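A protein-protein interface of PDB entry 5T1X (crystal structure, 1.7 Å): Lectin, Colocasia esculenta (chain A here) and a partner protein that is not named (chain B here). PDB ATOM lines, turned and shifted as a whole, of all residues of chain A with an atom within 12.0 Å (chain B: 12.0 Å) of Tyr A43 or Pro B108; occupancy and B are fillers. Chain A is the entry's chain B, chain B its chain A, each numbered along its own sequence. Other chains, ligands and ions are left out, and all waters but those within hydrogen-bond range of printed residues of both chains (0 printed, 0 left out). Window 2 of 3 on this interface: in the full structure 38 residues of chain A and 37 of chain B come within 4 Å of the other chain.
Of the printed residues of chain B, Leu A38 touches Ile B103 (3.6 Å) and Pro B105 (3.99 Å).
Of chain B, only Pro B105 (3.5 Å) comes within 4 Å of Gly A40.
Gly A41 touches just these residues of chain B: Pro B105 (3.8 Å) and Trp B106 (3.5 Å).
Lys A42 touches just these residues of chain B: Pro B105 (3.0 Å) and Trp B106 (3.7 Å).
Tyr A43 touches just these residues of chain B: Pro B105, Trp B106, Val B107 and Pro B108.
Printed residues of chain B within 4 Å of Gly A44: Pro B105 (3.6 Å).
Printed residues of chain B within 4 Å of Trp A45: Ile B103 (3.4 Å).
Ser A47 touches none of the printed residues of chain B.
Of the printed residues of chain B, Gly A96 touches Pro B105 (3.3 Å).
Of the printed residues of chain B, Ala A98 touches Lys B102 and Ile B103.
Of the printed residues of chain A, Ile B103 touches Leu A38 (3.6 Å), Trp A45 (3.4 Å), Phe A97 (3.5 Å) and Ala A98 (2.8 Å).
Trp B106 touches just these residues of chain A: Gly A41, Lys A42, Tyr A43, Asp A95 and Phe A97.
Of chain A, only Tyr A43 (3.8 Å) comes within 4 Å of Val B107.
Of chain A, only Tyr A43 (3.7 Å) comes within 4 Å of Pro B108.
The nearest residue of chain A that does not touch Pro B108 is Lys A42 (7.2 Å).
The backbone NH (N) of Ile B103 sits at hydrogen-bond distance from the backbone carbonyl oxygen (O) of Ala A98.
O of Pro B105 sits at hydrogen-bond distance from N of Tyr A43 (2.9 Å).
The backbone carbonyl oxygen (O) of Pro B105 sits at hydrogen-bond distance from the backbone NH (N) of Lys A42, 3.0 Å away.
NE1 of Trp B106 lies within hydrogen-bond range of O of Asp A95, 2.8 Å away.
The side-chain carboxylate (OD1) of Asp A95 sits close to the backbone NH (N) of Phe A97, at 3.5 Å.
The backbone NH of Leu A38 sits at hydrogen-bond distance from the backbone carbonyl oxygen of Trp A45, 2.8 Å away.
The backbone NH of Gly A96 sits at hydrogen-bond distance from a ring nitrogen (NE2) of His A26, at 3.3 Å.
The backbone NH of Trp B106 lies within hydrogen-bond range of the side-chain carboxylate of Asp B104 (2.9 Å).
A ring nitrogen (ND1) of His A26 lies within hydrogen-bond range of the backbone NH (N) of Gly A41 (3.4 Å).
The side-chain carboxylate (OD1) of Asp B104 is in hydrogen-bond range of the backbone NH (N) of Val B107 (3.2 Å).
Gly A41 touches Pro B105.
Gly A41 touches Trp B106.
Lys A42 touches Trp B106.
CD2 of Tyr A43 touches O of Val B107, 3.8 Å away.
Tyr A43 touches Pro B108.
Pro B105 touches Gly A44.
Lys B102 touches Phe A97 (CD to CD1, 3.7 Å).
Phe A97 touches Asp B104.
CD1 of Trp B106 touches CZ of Phe A97, 3.7 Å away.
O of Ala A98 touches CA of Lys B102 (3.5 Å).
Hydrophobic or aromatic side chains of chain B within 4 Å of the printed part of chain A: Ile B103, Pro B105, Trp B106 and Pro B108.
Of the 24 printed residues of chain A, 11 touch a printed residue of chain B.
Hydrophobic or aromatic side chains of chain A that line the printed part of chain B: Leu A38, Tyr A43, Trp A45 and Phe A97.
Among the printed residues, 21 pairs touch across the chains.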
ATOM      1  N   ASN A  25      40.738  30.528  16.577  1.00  0.00           N
ATOM      2  CA  ASN A  25      39.917  29.622  17.385  1.00  0.00           C
ATOM      3  C   ASN A  25      38.746  29.015  16.571  1.00  0.00           C
ATOM      4  O   ASN A  25      37.977  28.219  17.118  1.00  0.00           O
ATOM      5  CB  ASN A  25      39.389  30.335  18.642  1.00  0.00           C
ATOM      6  CG  ASN A  25      38.857  31.752  18.489  1.00  0.00           C
ATOM      7  OD1 ASN A  25      38.808  32.348  17.400  1.00  0.00           O
ATOM      8  ND2 ASN A  25      38.477  32.345  19.616  1.00  0.00           N
ATOM      9  N   HIS A  26      38.616  29.370  15.276  1.00  0.00           N
ATOM     10  CA  HIS A  26      37.537  28.851  14.418  1.00  0.00           C
ATOM     11  C   HIS A  26      37.912  27.530  13.752  1.00  0.00           C
ATOM     12  O   HIS A  26      39.073  27.321  13.400  1.00  0.00           O
ATOM     13  CB  HIS A  26      37.169  29.855  13.302  1.00  0.00           C
ATOM     14  CG  HIS A  26      37.074  31.282  13.754  1.00  0.00           C
ATOM     15  ND1 HIS A  26      36.140  31.681  14.691  1.00  0.00           N
ATOM     16  CD2 HIS A  26      37.799  32.360  13.370  1.00  0.00           C
ATOM     17  CE1 HIS A  26      36.330  32.980  14.865  1.00  0.00           C
ATOM     18  NE2 HIS A  26      37.312  33.438  14.087  1.00  0.00           N
ATOM     19  N   GLN A  27      36.915  26.656  13.533  1.00  0.00           N
ATOM     20  CA  GLN A  27      37.092  25.386  12.819  1.00  0.00           C
ATOM     21  C   GLN A  27      35.899  25.129  11.912  1.00  0.00           C
ATOM     22  O   GLN A  27      34.783  25.475  12.282  1.00  0.00           O
ATOM     23  CB  GLN A  27      37.236  24.184  13.779  1.00  0.00           C
ATOM     24  CG  GLN A  27      38.336  24.282  14.819  1.00  0.00           C
ATOM     25  CD  GLN A  27      38.261  23.094  15.743  1.00  0.00           C
ATOM     26  OE1 GLN A  27      38.673  21.986  15.396  1.00  0.00           O
ATOM     27  NE2 GLN A  27      37.676  23.283  16.916  1.00  0.00           N
ATOM     28  N   LEU A  28      36.126  24.510  10.754  1.00  0.00           N
ATOM     29  CA  LEU A  28      35.056  24.069   9.854  1.00  0.00           C
ATOM     30  C   LEU A  28      35.309  22.595   9.653  1.00  0.00           C
ATOM     31  O   LEU A  28      36.277  22.234   8.993  1.00  0.00           O
ATOM     32  CB  LEU A  28      34.989  24.864   8.523  1.00  0.00           C
ATOM     33  CG  LEU A  28      33.875  24.421   7.549  1.00  0.00           C
ATOM     34  CD1 LEU A  28      32.470  24.752   8.101  1.00  0.00           C
ATOM     35  CD2 LEU A  28      34.050  25.051   6.179  1.00  0.00           C
ATOM     36  N   GLN A  31      32.389  16.350   9.647  1.00  0.00           N
ATOM     37  CA  GLN A  31      32.378  15.276  10.626  1.00  0.00           C
ATOM     38  C   GLN A  31      31.990  13.912  10.072  1.00  0.00           C
ATOM     39  O   GLN A  31      31.320  13.810   9.043  1.00  0.00           O
ATOM     40  CB  GLN A  31      31.468  15.630  11.799  1.00  0.00           C
ATOM     41  CG  GLN A  31      31.824  16.969  12.425  1.00  0.00           C
ATOM     42  CD  GLN A  31      31.015  17.308  13.631  1.00  0.00           C
ATOM     43  OE1 GLN A  31      31.411  18.177  14.400  1.00  0.00           O
ATOM     44  NE2 GLN A  31      29.854  16.665  13.817  1.00  0.00           N
ATOM     45  N   ASN A  35      27.720  15.573   9.210  1.00  0.00           N
ATOM     46  CA  ASN A  35      27.388  16.951   9.514  1.00  0.00           C
ATOM     47  C   ASN A  35      28.588  17.862   9.308  1.00  0.00           C
ATOM     48  O   ASN A  35      29.670  17.572   9.823  1.00  0.00           O
ATOM     49  CB  ASN A  35      26.898  17.068  10.962  1.00  0.00           C
ATOM     50  CG  ASN A  35      25.994  18.246  11.221  1.00  0.00           C
ATOM     51  OD1 ASN A  35      25.337  18.791  10.323  1.00  0.00           O
ATOM     52  ND2 ASN A  35      25.876  18.609  12.478  1.00  0.00           N
ATOM     53  N   LEU A  36      28.400  18.946   8.551  1.00  0.00           N
ATOM     54  CA  LEU A  36      29.430  19.975   8.343  1.00  0.00           C
ATOM     55  C   LEU A  36      29.199  21.036   9.403  1.00  0.00           C
ATOM     56  O   LEU A  36      28.100  21.595   9.472  1.00  0.00           O
ATOM     57  CB  LEU A  36      29.376  20.562   6.925  1.00  0.00           C
ATOM     58  CG  LEU A  36      30.323  21.733   6.642  1.00  0.00           C
ATOM     59  CD1 LEU A  36      31.806  21.275   6.628  1.00  0.00           C
ATOM     60  CD2 LEU A  36      29.940  22.401   5.324  1.00  0.00           C
ATOM     61  N   VAL A  37      30.192  21.262  10.278  1.00  0.00           N
ATOM     62  CA  VAL A  37      29.991  22.173  11.397  1.00  0.00           C
ATOM     63  C   VAL A  37      31.052  23.257  11.465  1.00  0.00           C
ATOM     64  O   VAL A  37      32.248  22.977  11.463  1.00  0.00           O
ATOM     65  CB  VAL A  37      29.917  21.418  12.758  1.00  0.00           C
ATOM     66  CG1 VAL A  37      29.532  22.372  13.889  1.00  0.00           C
ATOM     67  CG2 VAL A  37      28.931  20.258  12.705  1.00  0.00           C
ATOM     68  N   LEU A  38      30.590  24.494  11.643  1.00  0.00           N
ATOM     69  CA  LEU A  38      31.485  25.602  11.876  1.00  0.00           C
ATOM     70  C   LEU A  38      31.501  25.849  13.374  1.00  0.00           C
ATOM     71  O   LEU A  38      30.488  26.272  13.940  1.00  0.00           O
ATOM     72  CB  LEU A  38      31.066  26.866  11.099  1.00  0.00           C
ATOM     73  CG  LEU A  38      32.164  27.942  10.893  1.00  0.00           C
ATOM     74  CD1 LEU A  38      31.744  28.946   9.846  1.00  0.00           C
ATOM     75  CD2 LEU A  38      32.503  28.688  12.172  1.00  0.00           C
ATOM     76  N   TYR A  39      32.640  25.556  14.019  1.00  0.00           N
ATOM     77  CA  TYR A  39      32.849  25.834  15.436  1.00  0.00           C
ATOM     78  C   TYR A  39      33.569  27.163  15.503  1.00  0.00           C
ATOM     79  O   TYR A  39      34.765  27.230  15.245  1.00  0.00           O
ATOM     80  CB  TYR A  39      33.666  24.702  16.103  1.00  0.00           C
ATOM     81  CG  TYR A  39      32.934  23.380  16.169  1.00  0.00           C
ATOM     82  CD1 TYR A  39      31.981  23.141  17.150  1.00  0.00           C
ATOM     83  CD2 TYR A  39      33.253  22.338  15.298  1.00  0.00           C
ATOM     84  CE1 TYR A  39      31.309  21.923  17.227  1.00  0.00           C
ATOM     85  CE2 TYR A  39      32.594  21.109  15.373  1.00  0.00           C
ATOM     86  CZ  TYR A  39      31.625  20.907  16.345  1.00  0.00           C
ATOM     87  OH  TYR A  39      30.961  19.707  16.466  1.00  0.00           O
ATOM     88  N   GLY A  40      32.824  28.234  15.731  1.00  0.00           N
ATOM     89  CA  GLY A  40      33.420  29.563  15.753  1.00  0.00           C
ATOM     90  C   GLY A  40      32.385  30.656  15.653  1.00  0.00           C
ATOM     91  O   GLY A  40      31.181  30.382  15.650  1.00  0.00           O
ATOM     92  N   GLY A  41      32.868  31.884  15.536  1.00  0.00           N
ATOM     93  CA  GLY A  41      32.013  33.059  15.512  1.00  0.00           C
ATOM     94  C   GLY A  41      31.376  33.209  16.876  1.00  0.00           C
ATOM     95  O   GLY A  41      32.015  32.911  17.893  1.00  0.00           O
ATOM     96  N   LYS A  42      30.108  33.615  16.914  1.00  0.00           N
ATOM     97  CA  LYS A  42      29.405  33.752  18.181  1.00  0.00           C
ATOM     98  C   LYS A  42      28.504  32.532  18.445  1.00  0.00           C
ATOM     99  O   LYS A  42      28.380  32.098  19.600  1.00  0.00           O
ATOM    100  CB  LYS A  42      28.568  35.050  18.185  1.00  0.00           C
ATOM    101  CG  LYS A  42      27.853  35.366  19.501  1.00  0.00           C
ATOM    102  CD  LYS A  42      28.789  35.789  20.626  1.00  0.00           C
ATOM    103  CE  LYS A  42      28.042  35.952  21.924  1.00  0.00           C
ATOM    104  NZ  LYS A  42      28.972  36.067  23.076  1.00  0.00           N
ATOM    105  N   TYR A  43      27.846  32.014  17.390  1.00  0.00           N
ATOM    106  CA  TYR A  43      26.849  30.947  17.534  1.00  0.00           C
ATOM    107  C   TYR A  43      27.153  29.662  16.777  1.00  0.00           C
ATOM    108  O   TYR A  43      26.436  28.664  16.951  1.00  0.00           O
ATOM    109  CB  TYR A  43      25.480  31.477  17.063  1.00  0.00           C
ATOM    110  CG  TYR A  43      25.042  32.722  17.805  1.00  0.00           C
ATOM    111  CD1 TYR A  43      24.808  32.693  19.180  1.00  0.00           C
ATOM    112  CD2 TYR A  43      24.906  33.938  17.145  1.00  0.00           C
ATOM    113  CE1 TYR A  43      24.427  33.840  19.872  1.00  0.00           C
ATOM    114  CE2 TYR A  43      24.522  35.093  17.829  1.00  0.00           C
ATOM    115  CZ  TYR A  43      24.294  35.040  19.193  1.00  0.00           C
ATOM    116  OH  TYR A  43      23.917  36.171  19.869  1.00  0.00           O
ATOM    117  N   GLY A  44      28.147  29.705  15.902  1.00  0.00           N
ATOM    118  CA  GLY A  44      28.486  28.566  15.067  1.00  0.00           C
ATOM    119  C   GLY A  44      27.464  28.395  13.961  1.00  0.00           C
ATOM    120  O   GLY A  44      26.566  29.227  13.792  1.00  0.00           O
ATOM    121  N   TRP A  45      27.591  27.303  13.215  1.00  0.00           N
ATOM    122  CA  TRP A  45      26.700  26.959  12.116  1.00  0.00           C
ATOM    123  C   TRP A  45      26.811  25.477  11.834  1.00  0.00           C
ATOM    124  O   TRP A  45      27.859  24.882  12.100  1.00  0.00           O
ATOM    125  CB  TRP A  45      27.090  27.776  10.864  1.00  0.00           C
ATOM    126  CG  TRP A  45      26.322  27.449   9.610  1.00  0.00           C
ATOM    127  CD1 TRP A  45      25.228  28.105   9.124  1.00  0.00           C
ATOM    128  CD2 TRP A  45      26.643  26.432   8.648  1.00  0.00           C
ATOM    129  NE1 TRP A  45      24.823  27.536   7.938  1.00  0.00           N
ATOM    130  CE2 TRP A  45      25.680  26.513   7.617  1.00  0.00           C
ATOM    131  CE3 TRP A  45      27.663  25.465   8.552  1.00  0.00           C
ATOM    132  CZ2 TRP A  45      25.685  25.644   6.518  1.00  0.00           C
ATOM    133  CZ3 TRP A  45      27.665  24.602   7.466  1.00  0.00           C
ATOM    134  CH2 TRP A  45      26.693  24.704   6.458  1.00  0.00           C
ATOM    135  N   GLN A  46      25.754  24.880  11.267  1.00  0.00           N
ATOM    136  CA  GLN A  46      25.821  23.475  10.849  1.00  0.00           C
ATOM    137  C   GLN A  46      24.949  23.230   9.623  1.00  0.00           C
ATOM    138  O   GLN A  46      23.977  23.951   9.396  1.00  0.00           O
ATOM    139  CB  GLN A  46      25.448  22.505  11.984  1.00  0.00           C
ATOM    140  CG  GLN A  46      24.007  22.616  12.478  1.00  0.00           C
ATOM    141  CD  GLN A  46      23.455  21.294  12.956  1.00  0.00           C
ATOM    142  OE1 GLN A  46      24.151  20.445  13.500  1.00  0.00           O
ATOM    143  NE2 GLN A  46      22.161  21.122  12.840  1.00  0.00           N
ATOM    144  N   SER A  47      25.313  22.225   8.819  1.00  0.00           N
ATOM    145  CA  SER A  47      24.516  21.861   7.645  1.00  0.00           C
ATOM    146  C   SER A  47      23.221  21.157   8.086  1.00  0.00           C
ATOM    147  O   SER A  47      22.279  21.084   7.300  1.00  0.00           O
ATOM    148  CB  SER A  47      25.327  20.966   6.715  1.00  0.00           C
ATOM    149  OG  SER A  47      25.760  19.814   7.415  1.00  0.00           O
ATOM    150  N   ASN A  48      23.175  20.651   9.347  1.00  0.00           N
ATOM    151  CA  ASN A  48      22.021  19.940   9.947  1.00  0.00           C
ATOM    152  C   ASN A  48      21.751  18.633   9.188  1.00  0.00           C
ATOM    153  O   ASN A  48      20.616  18.339   8.799  1.00  0.00           O
ATOM    154  CB  ASN A  48      20.757  20.847   9.990  1.00  0.00           C
ATOM    155  CG  ASN A  48      19.583  20.247  10.715  1.00  0.00           C
ATOM    156  OD1 ASN A  48      19.738  19.466  11.656  1.00  0.00           O
ATOM    157  ND2 ASN A  48      18.381  20.535  10.232  1.00  0.00           N
ATOM    158  N   LEU A  92      38.216  29.820   5.416  1.00  0.00           N
ATOM    159  CA  LEU A  92      37.742  29.984   6.783  1.00  0.00           C
ATOM    160  C   LEU A  92      38.508  31.196   7.260  1.00  0.00           C
ATOM    161  O   LEU A  92      39.708  31.100   7.550  1.00  0.00           O
ATOM    162  CB  LEU A  92      37.962  28.735   7.665  1.00  0.00           C
ATOM    163  CG  LEU A  92      37.522  28.897   9.142  1.00  0.00           C
ATOM    164  CD1 LEU A  92      36.015  29.134   9.271  1.00  0.00           C
ATOM    165  CD2 LEU A  92      37.978  27.715   9.987  1.00  0.00           C
ATOM    166  N   ASP A  95      38.030  36.209  10.703  1.00  0.00           N
ATOM    167  CA  ASP A  95      36.866  36.784  11.384  1.00  0.00           C
ATOM    168  C   ASP A  95      35.721  35.753  11.585  1.00  0.00           C
ATOM    169  O   ASP A  95      34.658  36.134  12.052  1.00  0.00           O
ATOM    170  CB  ASP A  95      36.362  38.058  10.666  1.00  0.00           C
ATOM    171  CG  ASP A  95      35.911  37.892   9.224  1.00  0.00           C
ATOM    172  OD1 ASP A  95      35.866  36.744   8.744  1.00  0.00           O
ATOM    173  OD2 ASP A  95      35.528  38.906   8.603  1.00  0.00           O
ATOM    174  N   GLY A  96      35.958  34.472  11.282  1.00  0.00           N
ATOM    175  CA  GLY A  96      34.983  33.414  11.535  1.00  0.00           C
ATOM    176  C   GLY A  96      34.046  33.050  10.402  1.00  0.00           C
ATOM    177  O   GLY A  96      33.455  31.967  10.422  1.00  0.00           O
ATOM    178  N   PHE A  97      33.879  33.949   9.428  1.00  0.00           N
ATOM    179  CA  PHE A  97      33.054  33.661   8.254  1.00  0.00           C
ATOM    180  C   PHE A  97      33.745  32.624   7.373  1.00  0.00           C
ATOM    181  O   PHE A  97      34.968  32.633   7.284  1.00  0.00           O
ATOM    182  CB  PHE A  97      32.840  34.937   7.421  1.00  0.00           C
ATOM    183  CG  PHE A  97      31.972  35.996   8.057  1.00  0.00           C
ATOM    184  CD1 PHE A  97      30.589  35.962   7.912  1.00  0.00           C
ATOM    185  CD2 PHE A  97      32.534  37.033   8.784  1.00  0.00           C
ATOM    186  CE1 PHE A  97      29.788  36.946   8.492  1.00  0.00           C
ATOM    187  CE2 PHE A  97      31.729  38.023   9.359  1.00  0.00           C
ATOM    188  CZ  PHE A  97      30.366  37.972   9.205  1.00  0.00           C
ATOM    189  N   ALA A  98      32.974  31.741   6.729  1.00  0.00           N
ATOM    190  CA  ALA A  98      33.534  30.802   5.744  1.00  0.00           C
ATOM    191  C   ALA A  98      32.967  31.249   4.417  1.00  0.00           C
ATOM    192  O   ALA A  98      31.741  31.327   4.273  1.00  0.00           O
ATOM    193  CB  ALA A  98      33.170  29.362   6.080  1.00  0.00           C
ATOM    194  N   LYS B 102      28.438  32.544   1.543  1.00  0.00           N
ATOM    195  CA  LYS B 102      28.985  32.873   2.854  1.00  0.00           C
ATOM    196  C   LYS B 102      28.245  32.108   3.947  1.00  0.00           C
ATOM    197  O   LYS B 102      27.017  32.027   3.912  1.00  0.00           O
ATOM    198  CB  LYS B 102      28.846  34.398   3.073  1.00  0.00           C
ATOM    199  CG  LYS B 102      29.399  34.934   4.398  1.00  0.00           C
ATOM    200  CD  LYS B 102      29.241  36.453   4.518  1.00  0.00           C
ATOM    201  CE  LYS B 102      27.889  36.872   5.054  1.00  0.00           C
ATOM    202  NZ  LYS B 102      27.753  38.352   5.123  1.00  0.00           N
ATOM    203  N   ILE B 103      29.002  31.511   4.880  1.00  0.00           N
ATOM    204  CA  ILE B 103      28.512  30.872   6.101  1.00  0.00           C
ATOM    205  C   ILE B 103      28.744  31.916   7.182  1.00  0.00           C
ATOM    206  O   ILE B 103      29.892  32.326   7.413  1.00  0.00           O
ATOM    207  CB  ILE B 103      29.180  29.507   6.427  1.00  0.00           C
ATOM    208  CG1 ILE B 103      28.822  28.420   5.389  1.00  0.00           C
ATOM    209  CG2 ILE B 103      28.781  29.053   7.832  1.00  0.00           C
ATOM    210  CD1 ILE B 103      29.723  27.142   5.454  1.00  0.00           C
ATOM    211  N   ASP B 104      27.662  32.344   7.844  1.00  0.00           N
ATOM    212  CA  ASP B 104      27.705  33.398   8.846  1.00  0.00           C
ATOM    213  C   ASP B 104      27.414  32.854  10.266  1.00  0.00           C
ATOM    214  O   ASP B 104      26.243  32.713  10.634  1.00  0.00           O
ATOM    215  CB  ASP B 104      26.691  34.492   8.461  1.00  0.00           C
ATOM    216  CG  ASP B 104      26.675  35.735   9.330  1.00  0.00           C
ATOM    217  OD1 ASP B 104      27.200  35.680  10.472  1.00  0.00           O
ATOM    218  OD2 ASP B 104      26.120  36.756   8.884  1.00  0.00           O
ATOM    219  N   PRO B 105      28.459  32.655  11.109  1.00  0.00           N
ATOM    220  CA  PRO B 105      28.213  32.162  12.479  1.00  0.00           C
ATOM    221  C   PRO B 105      28.038  33.303  13.502  1.00  0.00           C
ATOM    222  O   PRO B 105      28.183  33.074  14.703  1.00  0.00           O
ATOM    223  CB  PRO B 105      29.485  31.361  12.755  1.00  0.00           C
ATOM    224  CG  PRO B 105      30.562  32.173  12.081  1.00  0.00           C
ATOM    225  CD  PRO B 105      29.913  32.784  10.842  1.00  0.00           C
ATOM    226  N   TRP B 106      27.748  34.539  13.034  1.00  0.00           N
ATOM    227  CA  TRP B 106      27.620  35.705  13.916  1.00  0.00           C
ATOM    228  C   TRP B 106      26.181  36.201  14.099  1.00  0.00           C
ATOM    229  O   TRP B 106      25.855  36.713  15.175  1.00  0.00           O
ATOM    230  CB  TRP B 106      28.472  36.866  13.371  1.00  0.00           C
ATOM    231  CG  TRP B 106      29.940  36.589  13.391  1.00  0.00           C
ATOM    232  CD1 TRP B 106      30.700  36.137  12.357  1.00  0.00           C
ATOM    233  CD2 TRP B 106      30.808  36.672  14.524  1.00  0.00           C
ATOM    234  NE1 TRP B 106      32.001  35.971  12.765  1.00  0.00           N
ATOM    235  CE2 TRP B 106      32.100  36.307  14.089  1.00  0.00           C
ATOM    236  CE3 TRP B 106      30.636  37.097  15.856  1.00  0.00           C
ATOM    237  CZ2 TRP B 106      33.214  36.328  14.940  1.00  0.00           C
ATOM    238  CZ3 TRP B 106      31.734  37.087  16.707  1.00  0.00           C
ATOM    239  CH2 TRP B 106      33.002  36.701  16.248  1.00  0.00           C
ATOM    240  N   VAL B 107      25.346  36.089  13.057  1.00  0.00           N
ATOM    241  CA  VAL B 107      23.966  36.583  13.050  1.00  0.00           C
ATOM    242  C   VAL B 107      23.075  35.712  13.976  1.00  0.00           C
ATOM    243  O   VAL B 107      23.120  34.486  13.878  1.00  0.00           O
ATOM    244  CB  VAL B 107      23.423  36.677  11.586  1.00  0.00           C
ATOM    245  CG1 VAL B 107      23.334  35.315  10.894  1.00  0.00           C
ATOM    246  CG2 VAL B 107      22.099  37.423  11.509  1.00  0.00           C
ATOM    247  N   PRO B 108      22.289  36.320  14.897  1.00  0.00           N
ATOM    248  CA  PRO B 108      21.439  35.504  15.787  1.00  0.00           C
ATOM    249  C   PRO B 108      20.153  34.988  15.130  1.00  0.00           C
ATOM    250  O   PRO B 108      19.527  34.077  15.669  1.00  0.00           O
ATOM    251  CB  PRO B 108      21.103  36.465  16.928  1.00  0.00           C
ATOM    252  CG  PRO B 108      21.129  37.813  16.302  1.00  0.00           C
ATOM    253  CD  PRO B 108      22.141  37.766  15.184  1.00  0.00           C
ATOM    254  N   GLY B 109      19.761  35.590  14.006  1.00  0.00           N
ATOM    255  CA  GLY B 109      18.543  35.244  13.278  1.00  0.00           C
ATOM    256  C   GLY B 109      18.761  34.315  12.102  1.00  0.00           C
ATOM    257  O   GLY B 109      19.755  34.428  11.383  1.00  0.00           O
